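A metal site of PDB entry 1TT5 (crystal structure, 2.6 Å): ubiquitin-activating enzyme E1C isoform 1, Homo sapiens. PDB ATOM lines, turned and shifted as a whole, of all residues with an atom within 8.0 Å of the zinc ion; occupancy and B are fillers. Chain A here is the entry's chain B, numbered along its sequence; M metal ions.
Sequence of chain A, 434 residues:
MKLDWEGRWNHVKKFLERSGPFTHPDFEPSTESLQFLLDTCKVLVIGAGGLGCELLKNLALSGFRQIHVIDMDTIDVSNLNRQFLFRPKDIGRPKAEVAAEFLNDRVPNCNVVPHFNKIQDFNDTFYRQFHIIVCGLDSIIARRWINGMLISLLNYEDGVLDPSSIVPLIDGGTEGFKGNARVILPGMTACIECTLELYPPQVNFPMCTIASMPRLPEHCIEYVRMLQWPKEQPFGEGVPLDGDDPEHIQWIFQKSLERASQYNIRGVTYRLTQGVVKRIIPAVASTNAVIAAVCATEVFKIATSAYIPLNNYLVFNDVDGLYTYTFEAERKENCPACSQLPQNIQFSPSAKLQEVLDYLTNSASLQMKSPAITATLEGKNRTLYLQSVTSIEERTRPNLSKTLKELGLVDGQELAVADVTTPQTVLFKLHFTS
The guanidinium group of Arg 331 lies within hydrogen-bond range of the backbone carbonyl oxygen of Cys 338, at 3.5 Å. SG of Cys 191 lies close to N of Glu 193 (3.1 Å). The side-chain sulfur (SG) of Cys 335 lies close to the backbone NH (N) of Ala 337. The backbone carbonyl oxygen (O) of Cys 191 is in hydrogen-bond range of the guanidinium group (NH2) of Arg 182 (3.4 Å). SG of Cys 191 sits close to ND2 of Asn 147 (3.4 Å). OG of Ser 339 sits at hydrogen-bond distance from O of Cys 335 (2.6 Å). SG of Cys 194 sits close to N of Lys 332, at 3.3 Å.
The zinc ion is bound by SG of Cys 338 (2.2 Å), SG of Cys 335 (2.4 Å), SG of Cys 194 (2.4 Å) and SG of Cys 191 (2.6 Å).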
ATOM      1  N   ASN A 147     -11.887  -1.830  -3.396  1.00  0.00           N
ATOM      2  CA  ASN A 147     -11.608  -1.147  -4.658  1.00  0.00           C
ATOM      3  C   ASN A 147     -12.923  -0.636  -5.199  1.00  0.00           C
ATOM      4  O   ASN A 147     -13.015   0.506  -5.643  1.00  0.00           O
ATOM      5  CB  ASN A 147     -10.955  -2.104  -5.666  1.00  0.00           C
ATOM      6  CG  ASN A 147     -10.811  -1.477  -7.055  1.00  0.00           C
ATOM      7  OD1 ASN A 147     -10.034  -0.544  -7.259  1.00  0.00           O
ATOM      8  ND2 ASN A 147     -11.570  -1.979  -8.009  1.00  0.00           N
ATOM      9  N   ILE A 151     -14.372   3.397  -5.701  1.00  0.00           N
ATOM     10  CA  ILE A 151     -14.783   3.802  -7.036  1.00  0.00           C
ATOM     11  C   ILE A 151     -16.168   4.420  -6.903  1.00  0.00           C
ATOM     12  O   ILE A 151     -16.451   5.454  -7.505  1.00  0.00           O
ATOM     13  CB  ILE A 151     -14.907   2.616  -8.013  1.00  0.00           C
ATOM     14  CG1 ILE A 151     -13.556   1.895  -8.186  1.00  0.00           C
ATOM     15  CG2 ILE A 151     -15.447   3.125  -9.325  1.00  0.00           C
ATOM     16  CD1 ILE A 151     -12.492   2.769  -8.699  1.00  0.00           C
ATOM     17  N   ARG A 182       1.083  -0.844  -4.398  1.00  0.00           N
ATOM     18  CA  ARG A 182       0.598  -0.064  -5.509  1.00  0.00           C
ATOM     19  C   ARG A 182      -0.271   1.070  -5.072  1.00  0.00           C
ATOM     20  O   ARG A 182      -0.934   0.999  -4.035  1.00  0.00           O
ATOM     21  CB  ARG A 182      -0.176  -0.955  -6.490  1.00  0.00           C
ATOM     22  CG  ARG A 182      -1.506  -1.383  -5.999  1.00  0.00           C
ATOM     23  CD  ARG A 182      -2.200  -2.250  -7.037  1.00  0.00           C
ATOM     24  NE  ARG A 182      -2.655  -1.487  -8.196  1.00  0.00           N
ATOM     25  CZ  ARG A 182      -3.350  -2.018  -9.201  1.00  0.00           C
ATOM     26  NH1 ARG A 182      -3.667  -3.312  -9.168  1.00  0.00           N
ATOM     27  NH2 ARG A 182      -3.765  -1.246 -10.211  1.00  0.00           N
ATOM     28  N   ILE A 184      -3.374   3.466  -6.123  1.00  0.00           N
ATOM     29  CA  ILE A 184      -4.563   3.531  -6.963  1.00  0.00           C
ATOM     30  C   ILE A 184      -5.274   4.854  -6.718  1.00  0.00           C
ATOM     31  O   ILE A 184      -5.645   5.184  -5.599  1.00  0.00           O
ATOM     32  CB  ILE A 184      -5.592   2.418  -6.633  1.00  0.00           C
ATOM     33  CG1 ILE A 184      -5.131   1.037  -7.110  1.00  0.00           C
ATOM     34  CG2 ILE A 184      -6.900   2.739  -7.280  1.00  0.00           C
ATOM     35  CD1 ILE A 184      -4.173   0.399  -6.180  1.00  0.00           C
ATOM     36  N   GLY A 187     -10.532   6.475 -10.462  1.00  0.00           N
ATOM     37  CA  GLY A 187     -10.969   7.355 -11.531  1.00  0.00           C
ATOM     38  C   GLY A 187      -9.872   8.101 -12.278  1.00  0.00           C
ATOM     39  O   GLY A 187     -10.181   8.945 -13.113  1.00  0.00           O
ATOM     40  N   THR A 189      -6.302   6.390 -12.316  1.00  0.00           N
ATOM     41  CA  THR A 189      -5.340   5.367 -12.706  1.00  0.00           C
ATOM     42  C   THR A 189      -5.977   3.998 -12.671  1.00  0.00           C
ATOM     43  O   THR A 189      -7.153   3.848 -12.324  1.00  0.00           O
ATOM     44  CB  THR A 189      -4.141   5.377 -11.747  1.00  0.00           C
ATOM     45  OG1 THR A 189      -4.484   4.669 -10.547  1.00  0.00           O
ATOM     46  CG2 THR A 189      -3.775   6.801 -11.394  1.00  0.00           C
ATOM     47  N   ALA A 190      -5.202   2.988 -13.036  1.00  0.00           N
ATOM     48  CA  ALA A 190      -5.678   1.626 -13.028  1.00  0.00           C
ATOM     49  C   ALA A 190      -6.195   1.229 -11.639  1.00  0.00           C
ATOM     50  O   ALA A 190      -5.510   1.421 -10.632  1.00  0.00           O
ATOM     51  CB  ALA A 190      -4.551   0.682 -13.450  1.00  0.00           C
ATOM     52  N   CYS A 191      -7.398   0.672 -11.576  1.00  0.00           N
ATOM     53  CA  CYS A 191      -7.922   0.229 -10.295  1.00  0.00           C
ATOM     54  C   CYS A 191      -7.606  -1.268 -10.212  1.00  0.00           C
ATOM     55  O   CYS A 191      -7.011  -1.809 -11.132  1.00  0.00           O
ATOM     56  CB  CYS A 191      -9.439   0.478 -10.211  1.00  0.00           C
ATOM     57  SG  CYS A 191     -10.384  -0.841 -10.940  1.00  0.00           S
ATOM     58  N   ILE A 192      -7.990  -1.919  -9.118  1.00  0.00           N
ATOM     59  CA  ILE A 192      -7.731  -3.355  -8.928  1.00  0.00           C
ATOM     60  C   ILE A 192      -8.386  -4.186 -10.033  1.00  0.00           C
ATOM     61  O   ILE A 192      -7.818  -5.164 -10.532  1.00  0.00           O
ATOM     62  CB  ILE A 192      -8.267  -3.866  -7.534  1.00  0.00           C
ATOM     63  CG1 ILE A 192      -7.385  -3.355  -6.375  1.00  0.00           C
ATOM     64  CG2 ILE A 192      -8.378  -5.395  -7.566  1.00  0.00           C
ATOM     65  CD1 ILE A 192      -6.007  -3.807  -6.461  1.00  0.00           C
ATOM     66  N   GLU A 193      -9.594  -3.788 -10.422  1.00  0.00           N
ATOM     67  CA  GLU A 193     -10.358  -4.500 -11.449  1.00  0.00           C
ATOM     68  C   GLU A 193      -9.716  -4.372 -12.853  1.00  0.00           C
ATOM     69  O   GLU A 193      -9.929  -5.240 -13.713  1.00  0.00           O
ATOM     70  CB  GLU A 193     -11.804  -3.960 -11.435  1.00  0.00           C
ATOM     71  CG  GLU A 193     -12.918  -5.014 -11.284  1.00  0.00           C
ATOM     72  CD  GLU A 193     -12.737  -5.951 -10.091  1.00  0.00           C
ATOM     73  OE1 GLU A 193     -12.161  -7.050 -10.267  1.00  0.00           O
ATOM     74  OE2 GLU A 193     -13.174  -5.594  -8.975  1.00  0.00           O
ATOM     75  N   CYS A 194      -8.934  -3.315 -13.071  1.00  0.00           N
ATOM     76  CA  CYS A 194      -8.244  -3.096 -14.348  1.00  0.00           C
ATOM     77  C   CYS A 194      -7.098  -4.098 -14.576  1.00  0.00           C
ATOM     78  O   CYS A 194      -6.691  -4.338 -15.704  1.00  0.00           O
ATOM     79  CB  CYS A 194      -7.616  -1.705 -14.406  1.00  0.00           C
ATOM     80  SG  CYS A 194      -8.668  -0.305 -14.723  1.00  0.00           S
ATOM     81  N   THR A 195      -6.586  -4.673 -13.499  1.00  0.00           N
ATOM     82  CA  THR A 195      -5.447  -5.579 -13.620  1.00  0.00           C
ATOM     83  C   THR A 195      -5.634  -6.936 -12.965  1.00  0.00           C
ATOM     84  O   THR A 195      -4.734  -7.423 -12.289  1.00  0.00           O
ATOM     85  CB  THR A 195      -4.185  -4.911 -13.006  1.00  0.00           C
ATOM     86  OG1 THR A 195      -4.438  -4.540 -11.643  1.00  0.00           O
ATOM     87  CG2 THR A 195      -3.824  -3.650 -13.774  1.00  0.00           C
ATOM     88  N   GLU A 330      -1.979   0.010 -16.674  1.00  0.00           N
ATOM     89  CA  GLU A 330      -2.867   0.832 -17.488  1.00  0.00           C
ATOM     90  C   GLU A 330      -4.348   0.723 -17.102  1.00  0.00           C
ATOM     91  O   GLU A 330      -4.872  -0.367 -16.860  1.00  0.00           O
ATOM     92  CB  GLU A 330      -2.728   0.455 -18.972  1.00  0.00           C
ATOM     93  CG  GLU A 330      -1.392   0.798 -19.614  1.00  0.00           C
ATOM     94  CD  GLU A 330      -1.288   2.269 -19.991  1.00  0.00           C
ATOM     95  OE1 GLU A 330      -1.989   2.695 -20.942  1.00  0.00           O
ATOM     96  OE2 GLU A 330      -0.523   2.993 -19.326  1.00  0.00           O
ATOM     97  N   ARG A 331      -5.008   1.865 -17.053  1.00  0.00           N
ATOM     98  CA  ARG A 331      -6.420   1.878 -16.749  1.00  0.00           C
ATOM     99  C   ARG A 331      -7.128   1.296 -17.986  1.00  0.00           C
ATOM    100  O   ARG A 331      -7.058   1.869 -19.065  1.00  0.00           O
ATOM    101  CB  ARG A 331      -6.878   3.305 -16.510  1.00  0.00           C
ATOM    102  CG  ARG A 331      -8.346   3.431 -16.201  1.00  0.00           C
ATOM    103  CD  ARG A 331      -8.684   4.860 -15.922  1.00  0.00           C
ATOM    104  NE  ARG A 331     -10.061   5.031 -15.490  1.00  0.00           N
ATOM    105  CZ  ARG A 331     -10.650   6.211 -15.342  1.00  0.00           C
ATOM    106  NH1 ARG A 331      -9.964   7.321 -15.600  1.00  0.00           N
ATOM    107  NH2 ARG A 331     -11.919   6.275 -14.938  1.00  0.00           N
ATOM    108  N   LYS A 332      -7.782   0.156 -17.826  1.00  0.00           N
ATOM    109  CA  LYS A 332      -8.495  -0.492 -18.920  1.00  0.00           C
ATOM    110  C   LYS A 332      -9.768   0.322 -19.209  1.00  0.00           C
ATOM    111  O   LYS A 332     -10.498   0.695 -18.287  1.00  0.00           O
ATOM    112  CB  LYS A 332      -8.854  -1.921 -18.521  1.00  0.00           C
ATOM    113  CG  LYS A 332      -8.809  -2.929 -19.657  1.00  0.00           C
ATOM    114  CD  LYS A 332      -9.053  -4.356 -19.153  1.00  0.00           C
ATOM    115  CE  LYS A 332      -8.955  -5.389 -20.287  1.00  0.00           C
ATOM    116  NZ  LYS A 332      -8.997  -6.826 -19.815  1.00  0.00           N
ATOM    117  N   GLU A 333     -10.022   0.620 -20.469  1.00  0.00           N
ATOM    118  CA  GLU A 333     -11.207   1.406 -20.843  1.00  0.00           C
ATOM    119  C   GLU A 333     -12.502   0.615 -20.706  1.00  0.00           C
ATOM    120  O   GLU A 333     -13.574   1.182 -20.460  1.00  0.00           O
ATOM    121  CB  GLU A 333     -11.048   1.925 -22.281  1.00  0.00           C
ATOM    122  CG  GLU A 333      -9.840   2.827 -22.462  1.00  0.00           C
ATOM    123  CD  GLU A 333      -9.713   3.378 -23.880  1.00  0.00           C
ATOM    124  OE1 GLU A 333      -9.458   2.578 -24.811  1.00  0.00           O
ATOM    125  OE2 GLU A 333      -9.876   4.604 -24.055  1.00  0.00           O
ATOM    126  N   ASN A 334     -12.391  -0.698 -20.868  1.00  0.00           N
ATOM    127  CA  ASN A 334     -13.536  -1.607 -20.772  1.00  0.00           C
ATOM    128  C   ASN A 334     -13.708  -2.117 -19.343  1.00  0.00           C
ATOM    129  O   ASN A 334     -14.256  -3.195 -19.135  1.00  0.00           O
ATOM    130  CB  ASN A 334     -13.298  -2.798 -21.706  1.00  0.00           C
ATOM    131  CG  ASN A 334     -11.958  -3.509 -21.423  1.00  0.00           C
ATOM    132  OD1 ASN A 334     -11.818  -4.200 -20.413  1.00  0.00           O
ATOM    133  ND2 ASN A 334     -10.988  -3.328 -22.317  1.00  0.00           N
ATOM    134  N   CYS A 335     -13.267  -1.341 -18.368  1.00  0.00           N
ATOM    135  CA  CYS A 335     -13.344  -1.773 -16.985  1.00  0.00           C
ATOM    136  C   CYS A 335     -14.728  -1.821 -16.343  1.00  0.00           C
ATOM    137  O   CYS A 335     -15.432  -0.812 -16.256  1.00  0.00           O
ATOM    138  CB  CYS A 335     -12.410  -0.950 -16.082  1.00  0.00           C
ATOM    139  SG  CYS A 335     -12.092  -1.783 -14.493  1.00  0.00           S
ATOM    140  N   PRO A 336     -15.111  -3.008 -15.875  1.00  0.00           N
ATOM    141  CA  PRO A 336     -16.395  -3.289 -15.223  1.00  0.00           C
ATOM    142  C   PRO A 336     -16.581  -2.444 -13.961  1.00  0.00           C
ATOM    143  O   PRO A 336     -17.700  -2.043 -13.627  1.00  0.00           O
ATOM    144  CB  PRO A 336     -16.283  -4.775 -14.894  1.00  0.00           C
ATOM    145  CG  PRO A 336     -15.417  -5.285 -15.997  1.00  0.00           C
ATOM    146  CD  PRO A 336     -14.353  -4.242 -16.088  1.00  0.00           C
ATOM    147  N   ALA A 337     -15.474  -2.183 -13.273  1.00  0.00           N
ATOM    148  CA  ALA A 337     -15.495  -1.435 -12.033  1.00  0.00           C
ATOM    149  C   ALA A 337     -15.325   0.080 -12.133  1.00  0.00           C
ATOM    150  O   ALA A 337     -16.118   0.807 -11.548  1.00  0.00           O
ATOM    151  CB  ALA A 337     -14.438  -1.988 -11.103  1.00  0.00           C
ATOM    152  N   CYS A 338     -14.308   0.554 -12.850  1.00  0.00           N
ATOM    153  CA  CYS A 338     -14.096   1.999 -12.895  1.00  0.00           C
ATOM    154  C   CYS A 338     -14.475   2.738 -14.164  1.00  0.00           C
ATOM    155  O   CYS A 338     -14.427   3.970 -14.184  1.00  0.00           O
ATOM    156  CB  CYS A 338     -12.644   2.340 -12.518  1.00  0.00           C
ATOM    157  SG  CYS A 338     -11.373   1.941 -13.736  1.00  0.00           S
ATOM    158  N   SER A 339     -14.837   2.017 -15.221  1.00  0.00           N
ATOM    159  CA  SER A 339     -15.232   2.714 -16.450  1.00  0.00           C
ATOM    160  C   SER A 339     -16.517   3.437 -16.103  1.00  0.00           C
ATOM    161  O   SER A 339     -17.148   3.146 -15.085  1.00  0.00           O
ATOM    162  CB  SER A 339     -15.505   1.741 -17.583  1.00  0.00           C
ATOM    163  OG  SER A 339     -16.747   1.104 -17.358  1.00  0.00           O
HETATM  164 ZN    ZN M   1     -10.706  -0.168 -13.383  1.00  0.00          ZN
